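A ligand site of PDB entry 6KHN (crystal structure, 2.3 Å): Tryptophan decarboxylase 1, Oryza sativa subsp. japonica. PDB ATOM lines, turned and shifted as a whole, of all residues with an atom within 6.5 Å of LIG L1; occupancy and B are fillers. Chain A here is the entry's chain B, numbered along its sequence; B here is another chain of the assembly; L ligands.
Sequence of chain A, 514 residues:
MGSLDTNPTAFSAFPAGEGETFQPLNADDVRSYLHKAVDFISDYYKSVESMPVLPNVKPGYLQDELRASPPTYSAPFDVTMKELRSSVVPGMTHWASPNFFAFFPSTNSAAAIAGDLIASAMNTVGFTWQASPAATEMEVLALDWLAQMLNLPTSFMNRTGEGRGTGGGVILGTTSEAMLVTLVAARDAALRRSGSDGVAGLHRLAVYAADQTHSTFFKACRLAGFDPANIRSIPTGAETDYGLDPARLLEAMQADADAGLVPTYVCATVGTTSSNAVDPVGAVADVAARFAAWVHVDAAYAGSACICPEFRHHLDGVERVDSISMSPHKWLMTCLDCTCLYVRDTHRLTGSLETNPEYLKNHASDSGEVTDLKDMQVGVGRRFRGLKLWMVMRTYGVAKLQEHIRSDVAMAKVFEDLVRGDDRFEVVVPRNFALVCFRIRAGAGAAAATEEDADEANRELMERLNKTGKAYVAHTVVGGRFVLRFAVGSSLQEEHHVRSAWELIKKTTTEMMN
O1 of LIG L1 sits close to N of Ser 106 (3.4 Å).
O of Pro 105 is in hydrogen-bond range of O1 of LIG L1 (3.3 Å).
The side-chain amino group (NZ) of Lys 330 is covalently linked to a carbon (C5) of LG2 L2 (1.4 Å).
OG1 of Thr 273 sits at hydrogen-bond distance from O1 of LG2 L2, at 3.0 Å.
A nitrogen (N2) of LIG L1 is bonded to the side-chain hydroxyl (OH) of Tyr 359 of chain B (1.3 Å).
O of Phe 104 lies within hydrogen-bond range of O1 of LIG L1, 3.0 Å away.
O4 of LG2 L2 lies within hydrogen-bond range of N of Val 380 of chain B, at 3.3 Å.
The backbone NH of Gly 381 of chain B is in hydrogen-bond range of an oxygen (O5) of LG2 L2 (2.6 Å).
NE2 of His 214 is in hydrogen-bond range of N2 of LIG L1, at 3.3 Å.
A nitrogen (N1) of LIG L1 sits at hydrogen-bond distance from an oxygen (O5) of LG2 L2, 3.0 Å away.
NE2 of His 214 sits at hydrogen-bond distance from OH of Tyr 359 of chain B.
The backbone carbonyl oxygen (O) of Lys 330 is in hydrogen-bond range of the side-chain hydroxyl (OG1) of Thr 107 (2.7 Å).
Trp 95 touches LIG L1 (CZ3 to O1, 3.96 Å).
CD2 of His 329 touches C2 of LIG L1, at 3.6 Å.
Lys 330 touches LIG L1.
Val 125 of chain B touches LIG L1.
CE2 of Phe 127 of chain B touches C10 of LIG L1, 3.6 Å away.
N of Gly 381 of chain B touches N1 of LIG L1 (3.6 Å).
Within 4 Å of LIG L1: Trp 95, Phe 104, Pro 105, Ser 106, His 214, His 329, Lys 330, Val 125 of chain B, Phe 127 of chain B, Tyr 359 of chain B and Gly 381 of chain B.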
ATOM      1  N   TRP A  95     -12.950  26.182 -32.687  1.00  0.00           N
ATOM      2  CA  TRP A  95     -12.807  25.292 -31.533  1.00  0.00           C
ATOM      3  C   TRP A  95     -12.894  23.818 -31.942  1.00  0.00           C
ATOM      4  O   TRP A  95     -12.223  22.973 -31.341  1.00  0.00           O
ATOM      5  CB  TRP A  95     -13.884  25.623 -30.499  1.00  0.00           C
ATOM      6  CG  TRP A  95     -13.539  26.879 -29.678  1.00  0.00           C
ATOM      7  CD1 TRP A  95     -13.572  28.179 -30.123  1.00  0.00           C
ATOM      8  CD2 TRP A  95     -13.082  26.926 -28.329  1.00  0.00           C
ATOM      9  NE1 TRP A  95     -13.179  29.035 -29.109  1.00  0.00           N
ATOM     10  CE2 TRP A  95     -12.865  28.294 -27.998  1.00  0.00           C
ATOM     11  CE3 TRP A  95     -12.832  25.954 -27.344  1.00  0.00           C
ATOM     12  CZ2 TRP A  95     -12.421  28.701 -26.739  1.00  0.00           C
ATOM     13  CZ3 TRP A  95     -12.382  26.366 -26.092  1.00  0.00           C
ATOM     14  CH2 TRP A  95     -12.192  27.740 -25.793  1.00  0.00           C
ATOM     15  N   PHE A 103      -6.458  26.682 -24.515  1.00  0.00           N
ATOM     16  CA  PHE A 103      -7.390  26.751 -23.371  1.00  0.00           C
ATOM     17  C   PHE A 103      -7.661  25.322 -22.912  1.00  0.00           C
ATOM     18  O   PHE A 103      -6.710  24.564 -22.676  1.00  0.00           O
ATOM     19  CB  PHE A 103      -8.607  27.558 -23.799  1.00  0.00           C
ATOM     20  CG  PHE A 103      -8.259  28.884 -24.407  1.00  0.00           C
ATOM     21  CD1 PHE A 103      -7.551  29.836 -23.674  1.00  0.00           C
ATOM     22  CD2 PHE A 103      -8.608  29.176 -25.717  1.00  0.00           C
ATOM     23  CE1 PHE A 103      -7.208  31.055 -24.238  1.00  0.00           C
ATOM     24  CE2 PHE A 103      -8.275  30.405 -26.280  1.00  0.00           C
ATOM     25  CZ  PHE A 103      -7.580  31.355 -25.529  1.00  0.00           C
ATOM     26  N   PHE A 104      -8.920  24.906 -22.781  1.00  0.00           N
ATOM     27  CA  PHE A 104      -9.295  23.529 -22.737  1.00  0.00           C
ATOM     28  C   PHE A 104     -10.265  23.274 -23.878  1.00  0.00           C
ATOM     29  O   PHE A 104     -11.141  24.106 -24.129  1.00  0.00           O
ATOM     30  CB  PHE A 104      -9.954  23.150 -21.397  1.00  0.00           C
ATOM     31  CG  PHE A 104      -9.003  23.168 -20.243  1.00  0.00           C
ATOM     32  CD1 PHE A 104      -7.881  22.344 -20.234  1.00  0.00           C
ATOM     33  CD2 PHE A 104      -9.213  24.025 -19.163  1.00  0.00           C
ATOM     34  CE1 PHE A 104      -6.997  22.361 -19.167  1.00  0.00           C
ATOM     35  CE2 PHE A 104      -8.330  24.051 -18.090  1.00  0.00           C
ATOM     36  CZ  PHE A 104      -7.211  23.234 -18.093  1.00  0.00           C
ATOM     37  N   PRO A 105     -10.132  22.163 -24.601  1.00  0.00           N
ATOM     38  CA  PRO A 105     -11.022  21.916 -25.731  1.00  0.00           C
ATOM     39  C   PRO A 105     -12.446  21.674 -25.259  1.00  0.00           C
ATOM     40  O   PRO A 105     -12.696  21.109 -24.194  1.00  0.00           O
ATOM     41  CB  PRO A 105     -10.429  20.666 -26.400  1.00  0.00           C
ATOM     42  CG  PRO A 105      -9.683  19.973 -25.312  1.00  0.00           C
ATOM     43  CD  PRO A 105      -9.124  21.099 -24.442  1.00  0.00           C
ATOM     44  N   SER A 106     -13.401  22.138 -26.079  1.00  0.00           N
ATOM     45  CA  SER A 106     -14.814  21.928 -25.788  1.00  0.00           C
ATOM     46  C   SER A 106     -15.248  20.658 -26.508  1.00  0.00           C
ATOM     47  O   SER A 106     -15.832  20.688 -27.599  1.00  0.00           O
ATOM     48  CB  SER A 106     -15.636  23.139 -26.212  1.00  0.00           C
ATOM     49  OG  SER A 106     -15.318  23.510 -27.544  1.00  0.00           O
ATOM     50  N   THR A 107     -14.938  19.518 -25.884  1.00  0.00           N
ATOM     51  CA  THR A 107     -15.233  18.229 -26.506  1.00  0.00           C
ATOM     52  C   THR A 107     -16.741  18.073 -26.666  1.00  0.00           C
ATOM     53  O   THR A 107     -17.534  18.711 -25.974  1.00  0.00           O
ATOM     54  CB  THR A 107     -14.627  17.061 -25.693  1.00  0.00           C
ATOM     55  OG1 THR A 107     -15.262  16.908 -24.419  1.00  0.00           O
ATOM     56  CG2 THR A 107     -13.125  17.296 -25.470  1.00  0.00           C
ATOM     57  N   HIS A 214      -8.626  29.940 -10.537  1.00  0.00           N
ATOM     58  CA  HIS A 214      -9.047  30.830 -11.608  1.00  0.00           C
ATOM     59  C   HIS A 214      -9.422  32.190 -11.055  1.00  0.00           C
ATOM     60  O   HIS A 214     -10.010  32.292  -9.972  1.00  0.00           O
ATOM     61  CB  HIS A 214     -10.216  30.210 -12.372  1.00  0.00           C
ATOM     62  CG  HIS A 214     -10.388  30.787 -13.741  1.00  0.00           C
ATOM     63  ND1 HIS A 214     -10.867  32.054 -13.959  1.00  0.00           N
ATOM     64  CD2 HIS A 214     -10.131  30.262 -14.962  1.00  0.00           C
ATOM     65  CE1 HIS A 214     -10.896  32.302 -15.262  1.00  0.00           C
ATOM     66  NE2 HIS A 214     -10.455  31.228 -15.887  1.00  0.00           N
ATOM     67  N   THR A 273      -6.195  25.948 -14.375  1.00  0.00           N
ATOM     68  CA  THR A 273      -6.282  26.354 -15.776  1.00  0.00           C
ATOM     69  C   THR A 273      -4.895  26.556 -16.360  1.00  0.00           C
ATOM     70  O   THR A 273      -4.583  26.066 -17.459  1.00  0.00           O
ATOM     71  CB  THR A 273      -7.099  27.640 -15.883  1.00  0.00           C
ATOM     72  OG1 THR A 273      -8.435  27.395 -15.418  1.00  0.00           O
ATOM     73  CG2 THR A 273      -7.167  28.155 -17.329  1.00  0.00           C
ATOM     74  N   SER A 327     -17.143  20.226 -15.143  1.00  0.00           N
ATOM     75  CA  SER A 327     -17.822  20.666 -16.364  1.00  0.00           C
ATOM     76  C   SER A 327     -17.743  19.623 -17.462  1.00  0.00           C
ATOM     77  O   SER A 327     -16.726  19.511 -18.154  1.00  0.00           O
ATOM     78  CB  SER A 327     -17.220  21.986 -16.861  1.00  0.00           C
ATOM     79  OG  SER A 327     -17.624  23.054 -16.025  1.00  0.00           O
ATOM     80  N   HIS A 329     -18.954  20.004 -20.227  1.00  0.00           N
ATOM     81  CA  HIS A 329     -18.752  20.750 -21.455  1.00  0.00           C
ATOM     82  C   HIS A 329     -17.304  21.129 -21.696  1.00  0.00           C
ATOM     83  O   HIS A 329     -16.996  21.777 -22.704  1.00  0.00           O
ATOM     84  CB  HIS A 329     -19.670  21.993 -21.511  1.00  0.00           C
ATOM     85  CG  HIS A 329     -19.299  23.100 -20.578  1.00  0.00           C
ATOM     86  ND1 HIS A 329     -20.238  23.865 -19.928  1.00  0.00           N
ATOM     87  CD2 HIS A 329     -18.092  23.614 -20.232  1.00  0.00           C
ATOM     88  CE1 HIS A 329     -19.641  24.789 -19.202  1.00  0.00           C
ATOM     89  NE2 HIS A 329     -18.332  24.652 -19.363  1.00  0.00           N
ATOM     90  N   LYS A 330     -16.385  20.745 -20.805  1.00  0.00           N
ATOM     91  CA  LYS A 330     -14.983  20.704 -21.198  1.00  0.00           C
ATOM     92  C   LYS A 330     -14.630  19.300 -21.730  1.00  0.00           C
ATOM     93  O   LYS A 330     -14.642  19.085 -22.935  1.00  0.00           O
ATOM     94  CB  LYS A 330     -14.091  21.128 -20.038  1.00  0.00           C
ATOM     95  CG  LYS A 330     -14.299  22.606 -19.712  1.00  0.00           C
ATOM     96  CD  LYS A 330     -13.303  23.132 -18.721  1.00  0.00           C
ATOM     97  CE  LYS A 330     -13.292  24.669 -18.771  1.00  0.00           C
ATOM     98  NZ  LYS A 330     -13.225  25.316 -17.443  1.00  0.00           N
ATOM     99  N   TRP A 331     -14.398  18.335 -20.831  1.00  0.00           N
ATOM    100  CA  TRP A 331     -13.752  17.079 -21.197  1.00  0.00           C
ATOM    101  C   TRP A 331     -14.681  15.862 -21.143  1.00  0.00           C
ATOM    102  O   TRP A 331     -14.202  14.721 -21.033  1.00  0.00           O
ATOM    103  CB  TRP A 331     -12.548  16.853 -20.279  1.00  0.00           C
ATOM    104  CG  TRP A 331     -11.477  16.004 -20.846  1.00  0.00           C
ATOM    105  CD1 TRP A 331     -11.392  15.510 -22.104  1.00  0.00           C
ATOM    106  CD2 TRP A 331     -10.301  15.547 -20.151  1.00  0.00           C
ATOM    107  NE1 TRP A 331     -10.245  14.759 -22.245  1.00  0.00           N
ATOM    108  CE2 TRP A 331      -9.567  14.766 -21.060  1.00  0.00           C
ATOM    109  CE3 TRP A 331      -9.826  15.704 -18.847  1.00  0.00           C
ATOM    110  CZ2 TRP A 331      -8.368  14.144 -20.705  1.00  0.00           C
ATOM    111  CZ3 TRP A 331      -8.631  15.098 -18.498  1.00  0.00           C
ATOM    112  CH2 TRP A 331      -7.917  14.329 -19.428  1.00  0.00           C
ATOM    113  N   LEU A 336     -21.676  23.032 -24.594  1.00  0.00           N
ATOM    114  CA  LEU A 336     -22.081  24.061 -23.635  1.00  0.00           C
ATOM    115  C   LEU A 336     -23.603  24.290 -23.677  1.00  0.00           C
ATOM    116  O   LEU A 336     -24.232  24.165 -24.736  1.00  0.00           O
ATOM    117  CB  LEU A 336     -21.363  25.383 -23.928  1.00  0.00           C
ATOM    118  CG  LEU A 336     -19.908  25.581 -23.526  1.00  0.00           C
ATOM    119  CD1 LEU A 336     -18.972  24.810 -24.448  1.00  0.00           C
ATOM    120  CD2 LEU A 336     -19.553  27.093 -23.502  1.00  0.00           C
ATOM    121  N   VAL B 125     -16.477  28.918 -27.752  1.00  0.00           N
ATOM    122  CA  VAL B 125     -16.571  29.507 -26.420  1.00  0.00           C
ATOM    123  C   VAL B 125     -16.072  30.950 -26.523  1.00  0.00           C
ATOM    124  O   VAL B 125     -14.863  31.189 -26.662  1.00  0.00           O
ATOM    125  CB  VAL B 125     -15.755  28.719 -25.387  1.00  0.00           C
ATOM    126  CG1 VAL B 125     -15.997  29.286 -23.978  1.00  0.00           C
ATOM    127  CG2 VAL B 125     -16.100  27.238 -25.454  1.00  0.00           C
ATOM    128  N   PHE B 127     -15.407  33.735 -24.712  1.00  0.00           N
ATOM    129  CA  PHE B 127     -15.142  34.596 -23.565  1.00  0.00           C
ATOM    130  C   PHE B 127     -14.458  35.891 -23.971  1.00  0.00           C
ATOM    131  O   PHE B 127     -14.708  36.926 -23.362  1.00  0.00           O
ATOM    132  CB  PHE B 127     -14.305  33.855 -22.507  1.00  0.00           C
ATOM    133  CG  PHE B 127     -13.350  32.833 -23.069  1.00  0.00           C
ATOM    134  CD1 PHE B 127     -12.196  33.228 -23.724  1.00  0.00           C
ATOM    135  CD2 PHE B 127     -13.572  31.487 -22.873  1.00  0.00           C
ATOM    136  CE1 PHE B 127     -11.291  32.291 -24.209  1.00  0.00           C
ATOM    137  CE2 PHE B 127     -12.697  30.542 -23.372  1.00  0.00           C
ATOM    138  CZ  PHE B 127     -11.540  30.950 -24.045  1.00  0.00           C
ATOM    139  N   PRO B 357      -7.002  37.694 -16.560  1.00  0.00           N
ATOM    140  CA  PRO B 357      -6.056  36.580 -16.400  1.00  0.00           C
ATOM    141  C   PRO B 357      -5.072  36.503 -17.571  1.00  0.00           C
ATOM    142  O   PRO B 357      -5.409  36.778 -18.714  1.00  0.00           O
ATOM    143  CB  PRO B 357      -6.968  35.351 -16.358  1.00  0.00           C
ATOM    144  CG  PRO B 357      -8.147  35.753 -17.167  1.00  0.00           C
ATOM    145  CD  PRO B 357      -8.356  37.214 -16.888  1.00  0.00           C
ATOM    146  N   TYR B 359      -3.627  34.035 -19.165  1.00  0.00           N
ATOM    147  CA  TYR B 359      -3.801  33.071 -20.247  1.00  0.00           C
ATOM    148  C   TYR B 359      -4.826  33.527 -21.286  1.00  0.00           C
ATOM    149  O   TYR B 359      -4.827  32.991 -22.402  1.00  0.00           O
ATOM    150  CB  TYR B 359      -4.177  31.699 -19.670  1.00  0.00           C
ATOM    151  CG  TYR B 359      -5.644  31.526 -19.376  1.00  0.00           C
ATOM    152  CD1 TYR B 359      -6.237  32.145 -18.272  1.00  0.00           C
ATOM    153  CD2 TYR B 359      -6.448  30.721 -20.186  1.00  0.00           C
ATOM    154  CE1 TYR B 359      -7.575  31.980 -17.990  1.00  0.00           C
ATOM    155  CE2 TYR B 359      -7.792  30.550 -19.914  1.00  0.00           C
ATOM    156  CZ  TYR B 359      -8.363  31.192 -18.819  1.00  0.00           C
ATOM    157  OH  TYR B 359      -9.708  31.020 -18.547  1.00  0.00           O
ATOM    158  N   LEU B 360      -5.653  34.530 -20.961  1.00  0.00           N
ATOM    159  CA  LEU B 360      -6.629  35.089 -21.903  1.00  0.00           C
ATOM    160  C   LEU B 360      -6.123  36.320 -22.650  1.00  0.00           C
ATOM    161  O   LEU B 360      -6.824  36.797 -23.545  1.00  0.00           O
ATOM    162  CB  LEU B 360      -7.917  35.448 -21.158  1.00  0.00           C
ATOM    163  CG  LEU B 360      -8.708  34.206 -20.733  1.00  0.00           C
ATOM    164  CD1 LEU B 360     -10.090  34.569 -20.264  1.00  0.00           C
ATOM    165  CD2 LEU B 360      -8.767  33.190 -21.906  1.00  0.00           C
ATOM    166  N   VAL B 380     -17.108  32.939 -17.280  1.00  0.00           N
ATOM    167  CA  VAL B 380     -16.068  33.134 -18.279  1.00  0.00           C
ATOM    168  C   VAL B 380     -16.560  32.648 -19.630  1.00  0.00           C
ATOM    169  O   VAL B 380     -16.724  33.444 -20.571  1.00  0.00           O
ATOM    170  CB  VAL B 380     -14.761  32.418 -17.885  1.00  0.00           C
ATOM    171  CG1 VAL B 380     -13.644  32.777 -18.866  1.00  0.00           C
ATOM    172  CG2 VAL B 380     -14.398  32.754 -16.442  1.00  0.00           C
ATOM    173  N   GLY B 381     -16.814  31.338 -19.739  1.00  0.00           N
ATOM    174  CA  GLY B 381     -17.291  30.780 -20.985  1.00  0.00           C
ATOM    175  C   GLY B 381     -18.712  31.193 -21.314  1.00  0.00           C
ATOM    176  O   GLY B 381     -19.459  31.709 -20.472  1.00  0.00           O
ATOM    177  N   ARG B 382     -19.081  30.979 -22.580  1.00  0.00           N
ATOM    178  CA  ARG B 382     -20.410  31.343 -23.061  1.00  0.00           C
ATOM    179  C   ARG B 382     -20.634  30.773 -24.452  1.00  0.00           C
ATOM    180  O   ARG B 382     -19.712  30.695 -25.269  1.00  0.00           O
ATOM    181  CB  ARG B 382     -20.629  32.872 -23.090  1.00  0.00           C
ATOM    182  CG  ARG B 382     -19.649  33.663 -23.966  1.00  0.00           C
ATOM    183  CD  ARG B 382     -19.492  35.122 -23.481  1.00  0.00           C
ATOM    184  NE  ARG B 382     -20.789  35.738 -23.207  1.00  0.00           N
ATOM    185  CZ  ARG B 382     -21.597  36.214 -24.145  1.00  0.00           C
ATOM    186  NH1 ARG B 382     -21.242  36.143 -25.422  1.00  0.00           N
ATOM    187  NH2 ARG B 382     -22.770  36.740 -23.815  1.00  0.00           N
HETATM  188  O1  LIG L   1     -14.011  24.046 -23.334  1.00  0.00           O
HETATM  189  C1  LIG L   1     -14.266  25.131 -22.500  1.00  0.00           C
HETATM  190  C2  LIG L   1     -15.581  25.398 -22.121  1.00  0.00           C
HETATM  191  C3  LIG L   1     -15.863  26.475 -21.285  1.00  0.00           C
HETATM  192  C4  LIG L   1     -14.801  27.286 -20.818  1.00  0.00           C
HETATM  193  N1  LIG L   1     -14.770  28.393 -19.993  1.00  0.00           N
HETATM  194  C5  LIG L   1     -13.473  28.791 -19.861  1.00  0.00           C
HETATM  195  C6  LIG L   1     -12.681  27.937 -20.599  1.00  0.00           C
HETATM  196  C7  LIG L   1     -13.500  27.016 -21.195  1.00  0.00           C
HETATM  197  C8  LIG L   1     -13.217  25.929 -22.054  1.00  0.00           C
HETATM  198  C9  LIG L   1     -11.186  28.245 -20.551  1.00  0.00           C
HETATM  199  C10 LIG L   1     -11.100  29.745 -20.230  1.00  0.00           C
HETATM  200  N2  LIG L   1     -10.456  30.038 -18.951  1.00  0.00           N
HETATM  201  N1  LG2 L   2     -12.113  26.973 -13.345  1.00  0.00           N
HETATM  202  C1  LG2 L   2     -11.259  26.128 -14.025  1.00  0.00           C
HETATM  203  C2  LG2 L   2     -10.299  25.240 -13.287  1.00  0.00           C
HETATM  204  C3  LG2 L   2     -11.284  26.098 -15.408  1.00  0.00           C
HETATM  205  O1  LG2 L   2     -10.451  25.264 -16.128  1.00  0.00           O
HETATM  206  C4  LG2 L   2     -12.163  26.914 -16.111  1.00  0.00           C
HETATM  207  C5  LG2 L   2     -12.500  26.543 -17.532  1.00  0.00           C
HETATM  208  C6  LG2 L   2     -13.018  27.760 -15.431  1.00  0.00           C
HETATM  209  C7  LG2 L   2     -12.994  27.798 -14.042  1.00  0.00           C
HETATM  210  C8  LG2 L   2     -13.952  28.637 -16.235  1.00  0.00           C
HETATM  211  O2  LG2 L   2     -15.207  28.680 -15.612  1.00  0.00           O
HETATM  212  P1  LG2 L   2     -16.556  29.093 -16.394  1.00  0.00           P
HETATM  213  O3  LG2 L   2     -17.398  27.847 -16.573  1.00  0.00           O
HETATM  214  O4  LG2 L   2     -17.220  30.153 -15.528  1.00  0.00           O
HETATM  215  O5  LG2 L   2     -16.277  29.694 -17.747  1.00  0.00           O
